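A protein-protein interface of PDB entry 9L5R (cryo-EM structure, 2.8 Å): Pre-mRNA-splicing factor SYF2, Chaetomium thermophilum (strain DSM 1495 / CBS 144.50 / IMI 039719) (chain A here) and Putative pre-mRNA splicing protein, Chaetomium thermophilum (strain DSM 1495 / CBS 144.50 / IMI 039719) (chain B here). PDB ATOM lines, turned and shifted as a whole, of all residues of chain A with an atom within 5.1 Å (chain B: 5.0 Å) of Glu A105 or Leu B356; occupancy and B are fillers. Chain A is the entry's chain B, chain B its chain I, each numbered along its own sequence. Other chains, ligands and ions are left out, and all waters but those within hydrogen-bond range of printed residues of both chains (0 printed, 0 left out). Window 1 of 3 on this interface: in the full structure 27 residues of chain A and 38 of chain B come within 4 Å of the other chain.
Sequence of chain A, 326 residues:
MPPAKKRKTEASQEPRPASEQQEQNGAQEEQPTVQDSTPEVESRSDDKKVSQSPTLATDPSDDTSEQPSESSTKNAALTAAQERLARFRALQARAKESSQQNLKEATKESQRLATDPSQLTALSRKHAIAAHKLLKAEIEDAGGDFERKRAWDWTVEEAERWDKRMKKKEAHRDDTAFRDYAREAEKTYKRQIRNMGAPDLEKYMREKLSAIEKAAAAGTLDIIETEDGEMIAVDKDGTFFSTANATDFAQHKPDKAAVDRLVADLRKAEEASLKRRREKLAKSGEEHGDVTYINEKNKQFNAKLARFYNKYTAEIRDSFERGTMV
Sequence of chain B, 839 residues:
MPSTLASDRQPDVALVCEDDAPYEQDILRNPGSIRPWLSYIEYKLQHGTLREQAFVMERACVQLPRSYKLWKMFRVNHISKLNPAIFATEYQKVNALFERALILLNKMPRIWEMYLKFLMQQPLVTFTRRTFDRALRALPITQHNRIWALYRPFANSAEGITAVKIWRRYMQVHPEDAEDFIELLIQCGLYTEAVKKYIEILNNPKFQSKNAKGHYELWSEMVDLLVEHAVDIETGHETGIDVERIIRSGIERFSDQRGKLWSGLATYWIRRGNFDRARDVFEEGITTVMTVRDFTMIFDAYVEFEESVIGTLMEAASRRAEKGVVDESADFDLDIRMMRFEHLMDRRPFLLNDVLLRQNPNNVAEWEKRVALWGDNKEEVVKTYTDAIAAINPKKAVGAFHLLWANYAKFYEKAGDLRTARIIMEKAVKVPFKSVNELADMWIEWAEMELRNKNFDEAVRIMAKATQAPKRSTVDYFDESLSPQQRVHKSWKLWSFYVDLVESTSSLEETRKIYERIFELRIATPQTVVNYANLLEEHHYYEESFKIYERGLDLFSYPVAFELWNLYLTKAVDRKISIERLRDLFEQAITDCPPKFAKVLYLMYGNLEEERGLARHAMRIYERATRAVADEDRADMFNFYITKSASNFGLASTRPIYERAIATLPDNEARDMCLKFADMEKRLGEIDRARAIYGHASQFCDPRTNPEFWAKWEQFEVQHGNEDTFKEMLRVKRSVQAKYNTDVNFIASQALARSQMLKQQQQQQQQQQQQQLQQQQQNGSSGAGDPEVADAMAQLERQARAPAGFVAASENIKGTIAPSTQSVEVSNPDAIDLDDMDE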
ATOM      1  N   GLN A 101     -17.200  22.280  27.619  1.00  0.00           N
ATOM      2  CA  GLN A 101     -16.001  21.474  27.403  1.00  0.00           C
ATOM      3  C   GLN A 101     -14.742  22.333  27.426  1.00  0.00           C
ATOM      4  O   GLN A 101     -13.687  21.898  27.901  1.00  0.00           O
ATOM      5  CB  GLN A 101     -16.115  20.723  26.076  1.00  0.00           C
ATOM      6  CG  GLN A 101     -17.041  19.518  26.118  1.00  0.00           C
ATOM      7  CD  GLN A 101     -17.415  19.024  24.733  1.00  0.00           C
ATOM      8  OE1 GLN A 101     -17.091  19.658  23.728  1.00  0.00           O
ATOM      9  NE2 GLN A 101     -18.103  17.890  24.673  1.00  0.00           N
ATOM     10  N   ASN A 102     -14.838  23.570  26.951  1.00  0.00           N
ATOM     11  CA  ASN A 102     -13.685  24.454  26.948  1.00  0.00           C
ATOM     12  C   ASN A 102     -13.438  25.115  28.297  1.00  0.00           C
ATOM     13  O   ASN A 102     -12.290  25.449  28.601  1.00  0.00           O
ATOM     14  CB  ASN A 102     -13.857  25.498  25.854  1.00  0.00           C
ATOM     15  CG  ASN A 102     -13.516  24.951  24.478  1.00  0.00           C
ATOM     16  OD1 ASN A 102     -14.350  24.929  23.577  1.00  0.00           O
ATOM     17  ND2 ASN A 102     -12.277  24.506  24.315  1.00  0.00           N
ATOM     18  N   LEU A 103     -14.472  25.295  29.121  1.00  0.00           N
ATOM     19  CA  LEU A 103     -14.237  25.638  30.520  1.00  0.00           C
ATOM     20  C   LEU A 103     -13.516  24.496  31.226  1.00  0.00           C
ATOM     21  O   LEU A 103     -12.631  24.723  32.063  1.00  0.00           O
ATOM     22  CB  LEU A 103     -15.565  25.974  31.203  1.00  0.00           C
ATOM     23  CG  LEU A 103     -15.609  26.599  32.604  1.00  0.00           C
ATOM     24  CD1 LEU A 103     -16.848  27.475  32.711  1.00  0.00           C
ATOM     25  CD2 LEU A 103     -15.620  25.557  33.725  1.00  0.00           C
ATOM     26  N   LYS A 104     -13.866  23.255  30.879  1.00  0.00           N
ATOM     27  CA  LYS A 104     -13.118  22.113  31.397  1.00  0.00           C
ATOM     28  C   LYS A 104     -11.666  22.136  30.911  1.00  0.00           C
ATOM     29  O   LYS A 104     -10.740  21.852  31.680  1.00  0.00           O
ATOM     30  CB  LYS A 104     -13.809  20.810  31.003  1.00  0.00           C
ATOM     31  CG  LYS A 104     -15.185  20.601  31.629  1.00  0.00           C
ATOM     32  CD  LYS A 104     -16.078  19.767  30.718  1.00  0.00           C
ATOM     33  CE  LYS A 104     -17.548  19.900  31.079  1.00  0.00           C
ATOM     34  NZ  LYS A 104     -18.430  19.402  29.987  1.00  0.00           N
ATOM     35  N   GLU A 105     -11.450  22.496  29.641  1.00  0.00           N
ATOM     36  CA  GLU A 105     -10.091  22.635  29.115  1.00  0.00           C
ATOM     37  C   GLU A 105      -9.321  23.749  29.817  1.00  0.00           C
ATOM     38  O   GLU A 105      -8.100  23.646  30.004  1.00  0.00           O
ATOM     39  CB  GLU A 105     -10.134  22.883  27.610  1.00  0.00           C
ATOM     40  CG  GLU A 105     -10.148  21.607  26.784  1.00  0.00           C
ATOM     41  CD  GLU A 105      -9.748  21.839  25.344  1.00  0.00           C
ATOM     42  OE1 GLU A 105      -9.455  22.999  24.989  1.00  0.00           O
ATOM     43  OE2 GLU A 105      -9.732  20.862  24.566  1.00  0.00           O
ATOM     44  N   ALA A 106     -10.015  24.819  30.201  1.00  0.00           N
ATOM     45  CA  ALA A 106      -9.415  25.836  31.056  1.00  0.00           C
ATOM     46  C   ALA A 106      -9.034  25.266  32.415  1.00  0.00           C
ATOM     47  O   ALA A 106      -8.023  25.678  32.993  1.00  0.00           O
ATOM     48  CB  ALA A 106     -10.373  27.015  31.222  1.00  0.00           C
ATOM     49  N   THR A 107      -9.831  24.331  32.945  1.00  0.00           N
ATOM     50  CA  THR A 107      -9.461  23.706  34.215  1.00  0.00           C
ATOM     51  C   THR A 107      -8.260  22.775  34.067  1.00  0.00           C
ATOM     52  O   THR A 107      -7.515  22.580  35.051  1.00  0.00           O
ATOM     53  CB  THR A 107     -10.637  22.938  34.823  1.00  0.00           C
ATOM     54  OG1 THR A 107     -11.056  21.900  33.930  1.00  0.00           O
ATOM     55  CG2 THR A 107     -11.802  23.878  35.106  1.00  0.00           C
ATOM     56  N   LYS A 108      -8.062  22.197  32.857  1.00  0.00           N
ATOM     57  CA  LYS A 108      -6.818  21.472  32.540  1.00  0.00           C
ATOM     58  C   LYS A 108      -5.603  22.390  32.365  1.00  0.00           C
ATOM     59  O   LYS A 108      -4.519  22.052  32.876  1.00  0.00           O
ATOM     60  CB  LYS A 108      -6.899  20.570  31.296  1.00  0.00           C
ATOM     61  CG  LYS A 108      -7.479  19.158  31.477  1.00  0.00           C
ATOM     62  CD  LYS A 108      -8.960  18.975  31.640  1.00  0.00           C
ATOM     63  CE  LYS A 108      -9.637  19.265  30.326  1.00  0.00           C
ATOM     64  NZ  LYS A 108     -11.096  19.033  30.408  1.00  0.00           N
ATOM     65  N   GLU A 109      -5.775  23.579  31.771  1.00  0.00           N
ATOM     66  CA  GLU A 109      -4.711  24.593  31.801  1.00  0.00           C
ATOM     67  C   GLU A 109      -4.351  24.978  33.238  1.00  0.00           C
ATOM     68  O   GLU A 109      -3.229  24.723  33.705  1.00  0.00           O
ATOM     69  CB  GLU A 109      -5.121  25.831  31.004  1.00  0.00           C
ATOM     70  CG  GLU A 109      -4.873  25.729  29.507  1.00  0.00           C
ATOM     71  CD  GLU A 109      -5.175  27.028  28.786  1.00  0.00           C
ATOM     72  OE1 GLU A 109      -5.907  27.865  29.351  1.00  0.00           O
ATOM     73  OE2 GLU A 109      -4.661  27.225  27.667  1.00  0.00           O
ATOM     74  N   VAL B 292      -6.152  29.373  25.440  1.00  0.00           N
ATOM     75  CA  VAL B 292      -7.421  28.691  25.205  1.00  0.00           C
ATOM     76  C   VAL B 292      -8.561  29.417  25.907  1.00  0.00           C
ATOM     77  O   VAL B 292      -9.661  29.542  25.358  1.00  0.00           O
ATOM     78  CB  VAL B 292      -7.317  27.220  25.646  1.00  0.00           C
ATOM     79  CG1 VAL B 292      -8.628  26.487  25.419  1.00  0.00           C
ATOM     80  CG2 VAL B 292      -6.201  26.539  24.885  1.00  0.00           C
ATOM     81  N   LEU B 351      -9.226  25.704  15.068  1.00  0.00           N
ATOM     82  CA  LEU B 351      -8.561  26.850  15.675  1.00  0.00           C
ATOM     83  C   LEU B 351      -8.270  26.609  17.150  1.00  0.00           C
ATOM     84  O   LEU B 351      -7.271  27.117  17.670  1.00  0.00           O
ATOM     85  CB  LEU B 351      -9.421  28.100  15.494  1.00  0.00           C
ATOM     86  CG  LEU B 351      -9.824  28.402  14.050  1.00  0.00           C
ATOM     87  CD1 LEU B 351     -10.983  29.384  14.007  1.00  0.00           C
ATOM     88  CD2 LEU B 351      -8.636  28.934  13.265  1.00  0.00           C
ATOM     89  N   LEU B 352      -9.118  25.836  17.829  1.00  0.00           N
ATOM     90  CA  LEU B 352      -8.862  25.483  19.222  1.00  0.00           C
ATOM     91  C   LEU B 352      -7.612  24.619  19.346  1.00  0.00           C
ATOM     92  O   LEU B 352      -6.775  24.839  20.231  1.00  0.00           O
ATOM     93  CB  LEU B 352     -10.081  24.764  19.801  1.00  0.00           C
ATOM     94  CG  LEU B 352      -9.867  23.925  21.059  1.00  0.00           C
ATOM     95  CD1 LEU B 352      -9.602  24.834  22.242  1.00  0.00           C
ATOM     96  CD2 LEU B 352     -11.067  23.031  21.319  1.00  0.00           C
ATOM     97  N   ASN B 353      -7.465  23.638  18.453  1.00  0.00           N
ATOM     98  CA  ASN B 353      -6.260  22.815  18.440  1.00  0.00           C
ATOM     99  C   ASN B 353      -5.033  23.639  18.066  1.00  0.00           C
ATOM    100  O   ASN B 353      -3.938  23.405  18.590  1.00  0.00           O
ATOM    101  CB  ASN B 353      -6.434  21.644  17.474  1.00  0.00           C
ATOM    102  CG  ASN B 353      -7.407  20.603  17.986  1.00  0.00           C
ATOM    103  OD1 ASN B 353      -8.342  20.212  17.287  1.00  0.00           O
ATOM    104  ND2 ASN B 353      -7.193  20.148  19.214  1.00  0.00           N
ATOM    105  N   ASP B 354      -5.201  24.603  17.155  1.00  0.00           N
ATOM    106  CA  ASP B 354      -4.101  25.497  16.803  1.00  0.00           C
ATOM    107  C   ASP B 354      -3.664  26.340  17.996  1.00  0.00           C
ATOM    108  O   ASP B 354      -2.464  26.523  18.229  1.00  0.00           O
ATOM    109  CB  ASP B 354      -4.507  26.393  15.634  1.00  0.00           C
ATOM    110  CG  ASP B 354      -3.312  26.963  14.897  1.00  0.00           C
ATOM    111  OD1 ASP B 354      -2.273  26.276  14.827  1.00  0.00           O
ATOM    112  OD2 ASP B 354      -3.411  28.100  14.390  1.00  0.00           O
ATOM    113  N   VAL B 355      -4.626  26.854  18.764  1.00  0.00           N
ATOM    114  CA  VAL B 355      -4.312  27.622  19.966  1.00  0.00           C
ATOM    115  C   VAL B 355      -3.629  26.735  21.004  1.00  0.00           C
ATOM    116  O   VAL B 355      -2.678  27.158  21.672  1.00  0.00           O
ATOM    117  CB  VAL B 355      -5.594  28.281  20.514  1.00  0.00           C
ATOM    118  CG1 VAL B 355      -5.402  28.783  21.938  1.00  0.00           C
ATOM    119  CG2 VAL B 355      -6.019  29.428  19.613  1.00  0.00           C
ATOM    120  N   LEU B 356      -4.089  25.488  21.136  1.00  0.00           N
ATOM    121  CA  LEU B 356      -3.478  24.554  22.080  1.00  0.00           C
ATOM    122  C   LEU B 356      -2.031  24.237  21.710  1.00  0.00           C
ATOM    123  O   LEU B 356      -1.153  24.224  22.581  1.00  0.00           O
ATOM    124  CB  LEU B 356      -4.314  23.277  22.151  1.00  0.00           C
ATOM    125  CG  LEU B 356      -5.520  23.377  23.086  1.00  0.00           C
ATOM    126  CD1 LEU B 356      -6.669  22.500  22.624  1.00  0.00           C
ATOM    127  CD2 LEU B 356      -5.106  23.004  24.502  1.00  0.00           C
ATOM    128  N   LEU B 357      -1.756  24.000  20.425  1.00  0.00           N
ATOM    129  CA  LEU B 357      -0.379  23.727  20.024  1.00  0.00           C
ATOM    130  C   LEU B 357       0.486  24.981  20.040  1.00  0.00           C
ATOM    131  O   LEU B 357       1.706  24.872  20.187  1.00  0.00           O
ATOM    132  CB  LEU B 357      -0.338  23.062  18.642  1.00  0.00           C
ATOM    133  CG  LEU B 357      -0.861  23.753  17.379  1.00  0.00           C
ATOM    134  CD1 LEU B 357       0.213  24.559  16.650  1.00  0.00           C
ATOM    135  CD2 LEU B 357      -1.471  22.723  16.447  1.00  0.00           C
ATOM    136  N   ARG B 358      -0.110  26.165  19.877  1.00  0.00           N
ATOM    137  CA  ARG B 358       0.652  27.394  20.057  1.00  0.00           C
ATOM    138  C   ARG B 358       1.002  27.617  21.522  1.00  0.00           C
ATOM    139  O   ARG B 358       2.079  28.140  21.830  1.00  0.00           O
ATOM    140  CB  ARG B 358      -0.131  28.583  19.504  1.00  0.00           C
ATOM    141  CG  ARG B 358       0.398  29.108  18.183  1.00  0.00           C
ATOM    142  CD  ARG B 358       0.097  30.588  18.017  1.00  0.00           C
ATOM    143  NE  ARG B 358      -1.302  30.892  18.289  1.00  0.00           N
ATOM    144  CZ  ARG B 358      -2.285  30.749  17.410  1.00  0.00           C
ATOM    145  NH1 ARG B 358      -2.057  30.311  16.183  1.00  0.00           N
ATOM    146  NH2 ARG B 358      -3.528  31.055  17.771  1.00  0.00           N
ATOM    147  N   GLN B 359       0.098  27.242  22.429  1.00  0.00           N
ATOM    148  CA  GLN B 359       0.397  27.289  23.856  1.00  0.00           C
ATOM    149  C   GLN B 359       1.501  26.302  24.212  1.00  0.00           C
ATOM    150  O   GLN B 359       2.441  26.638  24.943  1.00  0.00           O
ATOM    151  CB  GLN B 359      -0.868  26.991  24.659  1.00  0.00           C
ATOM    152  CG  GLN B 359      -0.641  26.854  26.153  1.00  0.00           C
ATOM    153  CD  GLN B 359      -1.798  26.171  26.855  1.00  0.00           C
ATOM    154  OE1 GLN B 359      -1.822  26.071  28.082  1.00  0.00           O
ATOM    155  NE2 GLN B 359      -2.763  25.693  26.079  1.00  0.00           N
ATOM    156  N   ASN B 360       1.408  25.082  23.697  1.00  0.00           N
ATOM    157  CA  ASN B 360       2.441  24.083  23.935  1.00  0.00           C
ATOM    158  C   ASN B 360       2.713  23.294  22.660  1.00  0.00           C
ATOM    159  O   ASN B 360       1.897  22.452  22.266  1.00  0.00           O
ATOM    160  CB  ASN B 360       2.034  23.137  25.064  1.00  0.00           C
ATOM    161  CG  ASN B 360       3.199  22.315  25.582  1.00  0.00           C
ATOM    162  OD1 ASN B 360       4.343  22.508  25.172  1.00  0.00           O
ATOM    163  ND2 ASN B 360       2.910  21.389  26.488  1.00  0.00           N
ATOM    164  N   GLU B 366      -2.585  16.342  21.397  1.00  0.00           N
ATOM    165  CA  GLU B 366      -3.245  17.440  20.698  1.00  0.00           C
ATOM    166  C   GLU B 366      -3.021  17.363  19.195  1.00  0.00           C
ATOM    167  O   GLU B 366      -3.942  17.629  18.412  1.00  0.00           O
ATOM    168  CB  GLU B 366      -2.758  18.784  21.233  1.00  0.00           C
ATOM    169  CG  GLU B 366      -3.608  19.347  22.353  1.00  0.00           C
ATOM    170  CD  GLU B 366      -5.062  19.505  21.956  1.00  0.00           C
ATOM    171  OE1 GLU B 366      -5.330  19.973  20.828  1.00  0.00           O
ATOM    172  OE2 GLU B 366      -5.940  19.178  22.780  1.00  0.00           O
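The backbone NH (N) of Val B292 lies close to the side-chain carboxylate (OE2) of Glu A109 (3.4 Å). The side-chain carboxylate (OE2) of Glu A109 is in hydrogen-bond range of the side-chain amide nitrogen (NE2) of Gln B359.
The side-chain amide nitrogen (ND2) of Asn A102 lies within hydrogen-bond range of the side-chain carboxylate (OE1) of Glu A105 (3.3 Å).
Among the printed residues, merely in contact across the chains: Asn A102 with Leu B352 (3.4 Å), Glu A105 with Val B292 (3.6 Å), Glu A105 with Leu B352 (3.3 Å) and Glu A105 with Leu B356 (3.7 Å).
Of the printed residues of chain B, Asn A102 touches Leu B352. Lys A104 touches none of the printed residues of chain B. Of chain B, only Val B292, Leu B352 and Leu B356 come within 4 Å of Glu A105. Thr A107 touches none of the printed residues of chain B. Of the printed residues of chain B, Glu A109 touches Val B292 and Gln B359. Of the printed residues of chain A, Val B292 touches Glu A105 and Glu A109. Leu B356 touches one residue of chain A. Printed residues of chain A within 4 Å of Gln B359: Glu A109. The nearest residue of chain B that does not touch Glu A105 is Glu B366 (4.5 Å). The nearest printed residue of chain A that does not touch Leu B356 is Glu A109 (5.3 Å). The nearest printed residue of chain B that does not touch Glu A109 is Leu B356 (5.3 Å).
Among the printed residues, no Asp or Glu carboxylate lies within 4 Å of a Lys or Arg side-chain nitrogen of the other chain.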
